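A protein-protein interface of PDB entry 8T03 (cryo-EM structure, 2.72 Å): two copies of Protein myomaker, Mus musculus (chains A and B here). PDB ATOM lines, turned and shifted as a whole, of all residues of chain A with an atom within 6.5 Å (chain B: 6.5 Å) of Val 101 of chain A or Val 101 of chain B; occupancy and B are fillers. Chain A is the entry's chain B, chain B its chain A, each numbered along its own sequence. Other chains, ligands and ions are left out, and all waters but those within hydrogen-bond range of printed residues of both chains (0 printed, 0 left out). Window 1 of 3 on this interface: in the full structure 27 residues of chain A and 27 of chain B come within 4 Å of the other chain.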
ATOM      1  N   TYR A  72      25.433 -34.257  12.997  1.00  0.00           N
ATOM      2  CA  TYR A  72      24.528 -33.390  12.195  1.00  0.00           C
ATOM      3  C   TYR A  72      24.262 -32.079  12.945  1.00  0.00           C
ATOM      4  O   TYR A  72      24.420 -31.002  12.337  1.00  0.00           O
ATOM      5  CB  TYR A  72      23.204 -34.089  11.875  1.00  0.00           C
ATOM      6  CG  TYR A  72      22.225 -33.197  11.158  1.00  0.00           C
ATOM      7  CD1 TYR A  72      22.407 -32.874   9.824  1.00  0.00           C
ATOM      8  CD2 TYR A  72      21.148 -32.627  11.822  1.00  0.00           C
ATOM      9  CE1 TYR A  72      21.532 -32.032   9.156  1.00  0.00           C
ATOM     10  CE2 TYR A  72      20.263 -31.782  11.170  1.00  0.00           C
ATOM     11  CZ  TYR A  72      20.454 -31.483   9.831  1.00  0.00           C
ATOM     12  OH  TYR A  72      19.587 -30.656   9.180  1.00  0.00           O
ATOM     13  N   LEU A  76      25.433 -28.304  11.847  1.00  0.00           N
ATOM     14  CA  LEU A  76      24.323 -27.334  11.629  1.00  0.00           C
ATOM     15  C   LEU A  76      24.450 -26.165  12.617  1.00  0.00           C
ATOM     16  O   LEU A  76      24.112 -25.037  12.213  1.00  0.00           O
ATOM     17  CB  LEU A  76      22.969 -28.043  11.758  1.00  0.00           C
ATOM     18  CG  LEU A  76      21.733 -27.172  11.510  1.00  0.00           C
ATOM     19  CD1 LEU A  76      21.715 -26.608  10.096  1.00  0.00           C
ATOM     20  CD2 LEU A  76      20.460 -27.957  11.776  1.00  0.00           C
ATOM     21  N   TRP A  79      26.911 -23.839  11.132  1.00  0.00           N
ATOM     22  CA  TRP A  79      26.273 -23.162   9.970  1.00  0.00           C
ATOM     23  C   TRP A  79      25.396 -21.994  10.449  1.00  0.00           C
ATOM     24  O   TRP A  79      25.598 -20.878   9.931  1.00  0.00           O
ATOM     25  CB  TRP A  79      25.483 -24.157   9.107  1.00  0.00           C
ATOM     26  CG  TRP A  79      24.810 -23.519   7.933  1.00  0.00           C
ATOM     27  CD1 TRP A  79      23.499 -23.154   7.847  1.00  0.00           C
ATOM     28  CD2 TRP A  79      25.417 -23.131   6.686  1.00  0.00           C
ATOM     29  NE1 TRP A  79      23.244 -22.581   6.632  1.00  0.00           N
ATOM     30  CE2 TRP A  79      24.399 -22.552   5.895  1.00  0.00           C
ATOM     31  CE3 TRP A  79      26.712 -23.220   6.155  1.00  0.00           C
ATOM     32  CZ2 TRP A  79      24.640 -22.070   4.608  1.00  0.00           C
ATOM     33  CZ3 TRP A  79      26.948 -22.743   4.884  1.00  0.00           C
ATOM     34  CH2 TRP A  79      25.924 -22.175   4.122  1.00  0.00           C
ATOM     35  N   VAL A  80      24.479 -22.224  11.397  1.00  0.00           N
ATOM     36  CA  VAL A  80      23.488 -21.194  11.849  1.00  0.00           C
ATOM     37  C   VAL A  80      24.187 -20.109  12.684  1.00  0.00           C
ATOM     38  O   VAL A  80      23.643 -18.986  12.724  1.00  0.00           O
ATOM     39  CB  VAL A  80      22.273 -21.789  12.593  1.00  0.00           C
ATOM     40  CG1 VAL A  80      21.517 -22.787  11.728  1.00  0.00           C
ATOM     41  CG2 VAL A  80      22.623 -22.399  13.945  1.00  0.00           C
ATOM     42  N   PHE A  96      19.282 -19.497   2.811  1.00  0.00           N
ATOM     43  CA  PHE A  96      20.643 -19.877   3.275  1.00  0.00           C
ATOM     44  C   PHE A  96      20.532 -20.838   4.464  1.00  0.00           C
ATOM     45  O   PHE A  96      21.345 -21.774   4.502  1.00  0.00           O
ATOM     46  CB  PHE A  96      21.508 -18.653   3.595  1.00  0.00           C
ATOM     47  CG  PHE A  96      22.131 -18.003   2.385  1.00  0.00           C
ATOM     48  CD1 PHE A  96      23.003 -18.711   1.568  1.00  0.00           C
ATOM     49  CD2 PHE A  96      21.853 -16.682   2.062  1.00  0.00           C
ATOM     50  CE1 PHE A  96      23.574 -18.116   0.453  1.00  0.00           C
ATOM     51  CE2 PHE A  96      22.428 -16.088   0.947  1.00  0.00           C
ATOM     52  CZ  PHE A  96      23.287 -16.804   0.145  1.00  0.00           C
ATOM     53  N   THR A  97      19.562 -20.645   5.370  1.00  0.00           N
ATOM     54  CA  THR A  97      19.274 -21.595   6.482  1.00  0.00           C
ATOM     55  C   THR A  97      18.952 -22.977   5.899  1.00  0.00           C
ATOM     56  O   THR A  97      19.581 -23.958   6.340  1.00  0.00           O
ATOM     57  CB  THR A  97      18.144 -21.114   7.403  1.00  0.00           C
ATOM     58  OG1 THR A  97      18.491 -19.819   7.895  1.00  0.00           O
ATOM     59  CG2 THR A  97      17.896 -22.052   8.567  1.00  0.00           C
ATOM     60  N   MET A  98      18.025 -23.038   4.938  1.00  0.00           N
ATOM     61  CA  MET A  98      17.525 -24.296   4.314  1.00  0.00           C
ATOM     62  C   MET A  98      18.650 -24.979   3.521  1.00  0.00           C
ATOM     63  O   MET A  98      18.670 -26.224   3.502  1.00  0.00           O
ATOM     64  CB  MET A  98      16.340 -24.011   3.383  1.00  0.00           C
ATOM     65  CG  MET A  98      15.478 -25.225   3.081  1.00  0.00           C
ATOM     66  SD  MET A  98      14.477 -25.770   4.492  1.00  0.00           S
ATOM     67  CE  MET A  98      15.253 -27.346   4.849  1.00  0.00           C
ATOM     68  N   LEU A  99      19.538 -24.197   2.895  1.00  0.00           N
ATOM     69  CA  LEU A  99      20.703 -24.691   2.109  1.00  0.00           C
ATOM     70  C   LEU A  99      21.632 -25.509   3.015  1.00  0.00           C
ATOM     71  O   LEU A  99      21.985 -26.635   2.617  1.00  0.00           O
ATOM     72  CB  LEU A  99      21.426 -23.490   1.489  1.00  0.00           C
ATOM     73  CG  LEU A  99      22.675 -23.796   0.666  1.00  0.00           C
ATOM     74  CD1 LEU A  99      22.339 -24.527  -0.624  1.00  0.00           C
ATOM     75  CD2 LEU A  99      23.431 -22.509   0.369  1.00  0.00           C
ATOM     76  N   GLY A 100      22.007 -24.965   4.177  1.00  0.00           N
ATOM     77  CA  GLY A 100      22.821 -25.661   5.191  1.00  0.00           C
ATOM     78  C   GLY A 100      22.121 -26.904   5.708  1.00  0.00           C
ATOM     79  O   GLY A 100      22.753 -27.971   5.703  1.00  0.00           O
ATOM     80  N   VAL A 101      20.852 -26.770   6.112  1.00  0.00           N
ATOM     81  CA  VAL A 101      19.999 -27.880   6.640  1.00  0.00           C
ATOM     82  C   VAL A 101      20.056 -29.071   5.673  1.00  0.00           C
ATOM     83  O   VAL A 101      20.371 -30.184   6.138  1.00  0.00           O
ATOM     84  CB  VAL A 101      18.549 -27.412   6.886  1.00  0.00           C
ATOM     85  CG1 VAL A 101      17.563 -28.569   6.974  1.00  0.00           C
ATOM     86  CG2 VAL A 101      18.453 -26.547   8.134  1.00  0.00           C
ATOM     87  N   LEU A 102      19.770 -28.843   4.387  1.00  0.00           N
ATOM     88  CA  LEU A 102      19.586 -29.924   3.377  1.00  0.00           C
ATOM     89  C   LEU A 102      20.940 -30.502   2.945  1.00  0.00           C
ATOM     90  O   LEU A 102      21.016 -31.740   2.831  1.00  0.00           O
ATOM     91  CB  LEU A 102      18.789 -29.394   2.178  1.00  0.00           C
ATOM     92  CG  LEU A 102      17.328 -29.038   2.457  1.00  0.00           C
ATOM     93  CD1 LEU A 102      16.683 -28.412   1.230  1.00  0.00           C
ATOM     94  CD2 LEU A 102      16.525 -30.252   2.907  1.00  0.00           C
ATOM     95  N   THR A 103      21.964 -29.671   2.709  1.00  0.00           N
ATOM     96  CA  THR A 103      23.301 -30.139   2.240  1.00  0.00           C
ATOM     97  C   THR A 103      24.060 -30.847   3.372  1.00  0.00           C
ATOM     98  O   THR A 103      24.755 -31.836   3.059  1.00  0.00           O
ATOM     99  CB  THR A 103      24.141 -29.010   1.632  1.00  0.00           C
ATOM    100  OG1 THR A 103      24.235 -27.977   2.613  1.00  0.00           O
ATOM    101  CG2 THR A 103      23.560 -28.474   0.341  1.00  0.00           C
ATOM    102  N   ILE A 104      23.952 -30.375   4.622  1.00  0.00           N
ATOM    103  CA  ILE A 104      24.600 -31.022   5.807  1.00  0.00           C
ATOM    104  C   ILE A 104      23.905 -32.366   6.073  1.00  0.00           C
ATOM    105  O   ILE A 104      24.615 -33.317   6.451  1.00  0.00           O
ATOM    106  CB  ILE A 104      24.617 -30.097   7.047  1.00  0.00           C
ATOM    107  CG1 ILE A 104      25.466 -28.847   6.789  1.00  0.00           C
ATOM    108  CG2 ILE A 104      25.109 -30.834   8.289  1.00  0.00           C
ATOM    109  CD1 ILE A 104      25.284 -27.737   7.802  1.00  0.00           C
ATOM    110  N   ALA A 105      22.585 -32.451   5.864  1.00  0.00           N
ATOM    111  CA  ALA A 105      21.780 -33.682   6.061  1.00  0.00           C
ATOM    112  C   ALA A 105      22.262 -34.774   5.098  1.00  0.00           C
ATOM    113  O   ALA A 105      22.597 -35.869   5.587  1.00  0.00           O
ATOM    114  CB  ALA A 105      20.308 -33.399   5.887  1.00  0.00           C
ATOM    115  N   VAL A 106      22.320 -34.476   3.792  1.00  0.00           N
ATOM    116  CA  VAL A 106      22.714 -35.449   2.725  1.00  0.00           C
ATOM    117  C   VAL A 106      24.181 -35.841   2.923  1.00  0.00           C
ATOM    118  O   VAL A 106      24.470 -37.052   2.836  1.00  0.00           O
ATOM    119  CB  VAL A 106      22.469 -34.915   1.300  1.00  0.00           C
ATOM    120  CG1 VAL A 106      23.033 -35.849   0.233  1.00  0.00           C
ATOM    121  CG2 VAL A 106      20.992 -34.670   1.042  1.00  0.00           C
ATOM    122  N   TYR B  72      11.940 -38.173   3.728  1.00  0.00           N
ATOM    123  CA  TYR B  72      12.248 -36.948   4.514  1.00  0.00           C
ATOM    124  C   TYR B  72      11.783 -35.705   3.746  1.00  0.00           C
ATOM    125  O   TYR B  72      11.076 -34.866   4.342  1.00  0.00           O
ATOM    126  CB  TYR B  72      13.740 -36.838   4.837  1.00  0.00           C
ATOM    127  CG  TYR B  72      14.098 -35.553   5.539  1.00  0.00           C
ATOM    128  CD1 TYR B  72      13.768 -35.358   6.871  1.00  0.00           C
ATOM    129  CD2 TYR B  72      14.712 -34.509   4.864  1.00  0.00           C
ATOM    130  CE1 TYR B  72      14.063 -34.172   7.524  1.00  0.00           C
ATOM    131  CE2 TYR B  72      15.015 -33.315   5.502  1.00  0.00           C
ATOM    132  CZ  TYR B  72      14.689 -33.146   6.838  1.00  0.00           C
ATOM    133  OH  TYR B  72      14.987 -31.976   7.474  1.00  0.00           O
ATOM    134  N   LEU B  76       8.791 -33.104   4.801  1.00  0.00           N
ATOM    135  CA  LEU B  76       9.219 -31.692   5.002  1.00  0.00           C
ATOM    136  C   LEU B  76       8.496 -30.780   4.000  1.00  0.00           C
ATOM    137  O   LEU B  76       8.185 -29.639   4.389  1.00  0.00           O
ATOM    138  CB  LEU B  76      10.742 -31.579   4.877  1.00  0.00           C
ATOM    139  CG  LEU B  76      11.331 -30.185   5.109  1.00  0.00           C
ATOM    140  CD1 LEU B  76      11.043 -29.678   6.515  1.00  0.00           C
ATOM    141  CD2 LEU B  76      12.828 -30.181   4.848  1.00  0.00           C
ATOM    142  N   TRP B  79       5.173 -30.088   5.466  1.00  0.00           N
ATOM    143  CA  TRP B  79       5.353 -29.161   6.617  1.00  0.00           C
ATOM    144  C   TRP B  79       5.480 -27.712   6.119  1.00  0.00           C
ATOM    145  O   TRP B  79       4.719 -26.865   6.623  1.00  0.00           O
ATOM    146  CB  TRP B  79       6.546 -29.577   7.489  1.00  0.00           C
ATOM    147  CG  TRP B  79       6.776 -28.663   8.652  1.00  0.00           C
ATOM    148  CD1 TRP B  79       7.696 -27.660   8.727  1.00  0.00           C
ATOM    149  CD2 TRP B  79       6.052 -28.639   9.897  1.00  0.00           C
ATOM    150  NE1 TRP B  79       7.606 -27.023   9.934  1.00  0.00           N
ATOM    151  CE2 TRP B  79       6.608 -27.600  10.675  1.00  0.00           C
ATOM    152  CE3 TRP B  79       4.998 -29.392  10.433  1.00  0.00           C
ATOM    153  CZ2 TRP B  79       6.145 -27.300  11.958  1.00  0.00           C
ATOM    154  CZ3 TRP B  79       4.542 -29.095  11.699  1.00  0.00           C
ATOM    155  CH2 TRP B  79       5.109 -28.063  12.450  1.00  0.00           C
ATOM    156  N   VAL B  80       6.384 -27.435   5.169  1.00  0.00           N
ATOM    157  CA  VAL B  80       6.683 -26.042   4.701  1.00  0.00           C
ATOM    158  C   VAL B  80       5.518 -25.501   3.854  1.00  0.00           C
ATOM    159  O   VAL B  80       5.387 -24.262   3.798  1.00  0.00           O
ATOM    160  CB  VAL B  80       8.031 -25.914   3.960  1.00  0.00           C
ATOM    161  CG1 VAL B  80       9.198 -26.351   4.834  1.00  0.00           C
ATOM    162  CG2 VAL B  80       8.060 -26.635   2.617  1.00  0.00           C
ATOM    163  N   PHE B  96       9.328 -22.261  13.698  1.00  0.00           N
ATOM    164  CA  PHE B  96       8.374 -23.309  13.245  1.00  0.00           C
ATOM    165  C   PHE B  96       8.979 -24.081  12.068  1.00  0.00           C
ATOM    166  O   PHE B  96       8.782 -25.306  12.044  1.00  0.00           O
ATOM    167  CB  PHE B  96       6.994 -22.731  12.913  1.00  0.00           C
ATOM    168  CG  PHE B  96       6.117 -22.493  14.117  1.00  0.00           C
ATOM    169  CD1 PHE B  96       5.747 -23.545  14.946  1.00  0.00           C
ATOM    170  CD2 PHE B  96       5.656 -21.220  14.425  1.00  0.00           C
ATOM    171  CE1 PHE B  96       4.943 -23.327  16.056  1.00  0.00           C
ATOM    172  CE2 PHE B  96       4.850 -21.005  15.534  1.00  0.00           C
ATOM    173  CZ  PHE B  96       4.496 -22.058  16.347  1.00  0.00           C
ATOM    174  N   THR B  97       9.704 -23.417  11.156  1.00  0.00           N
ATOM    175  CA  THR B  97      10.454 -24.086  10.055  1.00  0.00           C
ATOM    176  C   THR B  97      11.456 -25.082  10.655  1.00  0.00           C
ATOM    177  O   THR B  97      11.441 -26.252  10.229  1.00  0.00           O
ATOM    178  CB  THR B  97      11.162 -23.091   9.124  1.00  0.00           C
ATOM    179  OG1 THR B  97      10.185 -22.182   8.617  1.00  0.00           O
ATOM    180  CG2 THR B  97      11.871 -23.772   7.971  1.00  0.00           C
ATOM    181  N   MET B  98      12.273 -24.629  11.612  1.00  0.00           N
ATOM    182  CA  MET B  98      13.359 -25.425  12.250  1.00  0.00           C
ATOM    183  C   MET B  98      12.763 -26.590  13.056  1.00  0.00           C
ATOM    184  O   MET B  98      13.403 -27.657  13.091  1.00  0.00           O
ATOM    185  CB  MET B  98      14.211 -24.545  13.173  1.00  0.00           C
ATOM    186  CG  MET B  98      15.585 -25.116  13.486  1.00  0.00           C
ATOM    187  SD  MET B  98      16.726 -25.069  12.078  1.00  0.00           S
ATOM    188  CE  MET B  98      16.904 -26.821  11.745  1.00  0.00           C
ATOM    189  N   LEU B  99      11.593 -26.388  13.675  1.00  0.00           N
ATOM    190  CA  LEU B  99      10.863 -27.413  14.474  1.00  0.00           C
ATOM    191  C   LEU B  99      10.509 -28.610  13.582  1.00  0.00           C
ATOM    192  O   LEU B  99      10.804 -29.747  13.995  1.00  0.00           O
ATOM    193  CB  LEU B  99       9.613 -26.767  15.080  1.00  0.00           C
ATOM    194  CG  LEU B  99       8.712 -27.675  15.913  1.00  0.00           C
ATOM    195  CD1 LEU B  99       9.380 -28.101  17.211  1.00  0.00           C
ATOM    196  CD2 LEU B  99       7.389 -26.979  16.197  1.00  0.00           C
ATOM    197  N   GLY B 100       9.908 -28.360  12.414  1.00  0.00           N
ATOM    198  CA  GLY B 100       9.588 -29.395  11.412  1.00  0.00           C
ATOM    199  C   GLY B 100      10.841 -30.086  10.908  1.00  0.00           C
ATOM    200  O   GLY B 100      10.869 -31.326  10.930  1.00  0.00           O
ATOM    201  N   VAL B 101      11.849 -29.308  10.497  1.00  0.00           N
ATOM    202  CA  VAL B 101      13.161 -29.805   9.980  1.00  0.00           C
ATOM    203  C   VAL B 101      13.739 -30.834  10.963  1.00  0.00           C
ATOM    204  O   VAL B 101      14.060 -31.952  10.514  1.00  0.00           O
ATOM    205  CB  VAL B 101      14.145 -28.645   9.722  1.00  0.00           C
ATOM    206  CG1 VAL B 101      15.595 -29.107   9.645  1.00  0.00           C
ATOM    207  CG2 VAL B 101      13.774 -27.876   8.464  1.00  0.00           C
ATOM    208  N   LEU B 102      13.858 -30.473  12.245  1.00  0.00           N
ATOM    209  CA  LEU B 102      14.582 -31.279  13.266  1.00  0.00           C
ATOM    210  C   LEU B 102      13.737 -32.481  13.713  1.00  0.00           C
ATOM    211  O   LEU B 102      14.327 -33.570  13.842  1.00  0.00           O
ATOM    212  CB  LEU B 102      14.974 -30.393  14.455  1.00  0.00           C
ATOM    213  CG  LEU B 102      16.028 -29.321  14.167  1.00  0.00           C
ATOM    214  CD1 LEU B 102      16.241 -28.433  15.382  1.00  0.00           C
ATOM    215  CD2 LEU B 102      17.352 -29.933  13.730  1.00  0.00           C
ATOM    216  N   THR B 103      12.428 -32.313  13.942  1.00  0.00           N
ATOM    217  CA  THR B 103      11.538 -33.411  14.423  1.00  0.00           C
ATOM    218  C   THR B 103      11.272 -34.428  13.303  1.00  0.00           C
ATOM    219  O   THR B 103      11.204 -35.630  13.632  1.00  0.00           O
ATOM    220  CB  THR B 103      10.227 -32.888  15.019  1.00  0.00           C
ATOM    221  OG1 THR B 103       9.604 -32.075  14.025  1.00  0.00           O
ATOM    222  CG2 THR B 103      10.433 -32.109  16.301  1.00  0.00           C
ATOM    223  N   ILE B 104      11.118 -33.986  12.047  1.00  0.00           N
ATOM    224  CA  ILE B 104      10.914 -34.893  10.872  1.00  0.00           C
ATOM    225  C   ILE B 104      12.215 -35.671  10.622  1.00  0.00           C
ATOM    226  O   ILE B 104      12.116 -36.858  10.258  1.00  0.00           O
ATOM    227  CB  ILE B 104      10.414 -34.133   9.620  1.00  0.00           C
ATOM    228  CG1 ILE B 104       9.033 -33.518   9.866  1.00  0.00           C
ATOM    229  CG2 ILE B 104      10.391 -35.035   8.391  1.00  0.00           C
ATOM    230  CD1 ILE B 104       8.604 -32.493   8.838  1.00  0.00           C
ATOM    231  N   ALA B 105      13.381 -35.042  10.825  1.00  0.00           N
ATOM    232  CA  ALA B 105      14.714 -35.664  10.641  1.00  0.00           C
ATOM    233  C   ALA B 105      14.879 -36.832  11.619  1.00  0.00           C
ATOM    234  O   ALA B 105      15.175 -37.946  11.145  1.00  0.00           O
ATOM    235  CB  ALA B 105      15.815 -34.643  10.806  1.00  0.00           C
ATOM    236  N   VAL B 106      14.669 -36.595  12.921  1.00  0.00           N
ATOM    237  CA  VAL B 106      14.845 -37.614  14.002  1.00  0.00           C
ATOM    238  C   VAL B 106      13.808 -38.725  13.816  1.00  0.00           C
ATOM    239  O   VAL B 106      14.202 -39.904  13.919  1.00  0.00           O
ATOM    240  CB  VAL B 106      14.767 -37.012  15.420  1.00  0.00           C
ATOM    241  CG1 VAL B 106      14.779 -38.090  16.500  1.00  0.00           C
ATOM    242  CG2 VAL B 106      15.891 -36.021  15.668  1.00  0.00           C
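O of Val 101 of chain B is in hydrogen-bond range of OH of Tyr 72 of chain B, at 3.2 Å. O of Val 101 of chain A lies within hydrogen-bond range of OH of Tyr 72 of chain A (3.2 Å).
Met 98 of chain B touches Leu 76 of chain A (CE to CD2, 3.7 Å). Met 98 of chain A touches Leu 76 of chain B (CE to CD2, 3.7 Å). Val 101 of chain B touches Met 98 of chain A (CG2 to CE, 3.9 Å). CG2 of Val 101 of chain A touches CE of Met 98 of chain B, 3.9 Å away. Val 101 of chain A touches Val 101 of chain B.
Val 101 of chain A touches two residues of chain B. Val 101 of chain B touches just these residues of chain A: Met 98 and Val 101. Of the printed residues of chain B, Leu 76 of chain A touches Met 98 (3.7 Å). Printed residues of chain A within 4 Å of Met 98 of chain B: Leu 76 and Val 101. Printed residues of chain B within 4 Å of Met 98 of chain A: Leu 76 and Val 101. Gly 100 of chain A touches none of the printed residues of chain B. The nearest residue of chain B that does not touch Val 101 of chain A is Tyr 72 of chain B (4.3 Å). The nearest residue of chain A that does not touch Val 101 of chain B is Tyr 72 of chain A (4.3 Å).
Printed residues of chain A that touch a printed residue of chain B: Leu 76, Met 98 and Val 101. Among the printed residues, 5 pairs touch across the chains. Among the printed residues, no Asp or Glu carboxylate lies within 4 Å of a Lys or Arg side-chain nitrogen of the other chain.
Leu 76 of chain A touches Met 98 of chain B, and with the chains exchanged Met 98 of chain A touches Leu 76 of chain B. Met 98 of chain A touches Val 101 of chain B, and with the chains exchanged Val 101 of chain A touches Met 98 of chain B. Val 101 of chain B touches its own counterpart, Val 101 of chain A. Of the 5 pairs that touch across the chains among the printed residues, 5 have their exchanged pair printed and touching as well.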
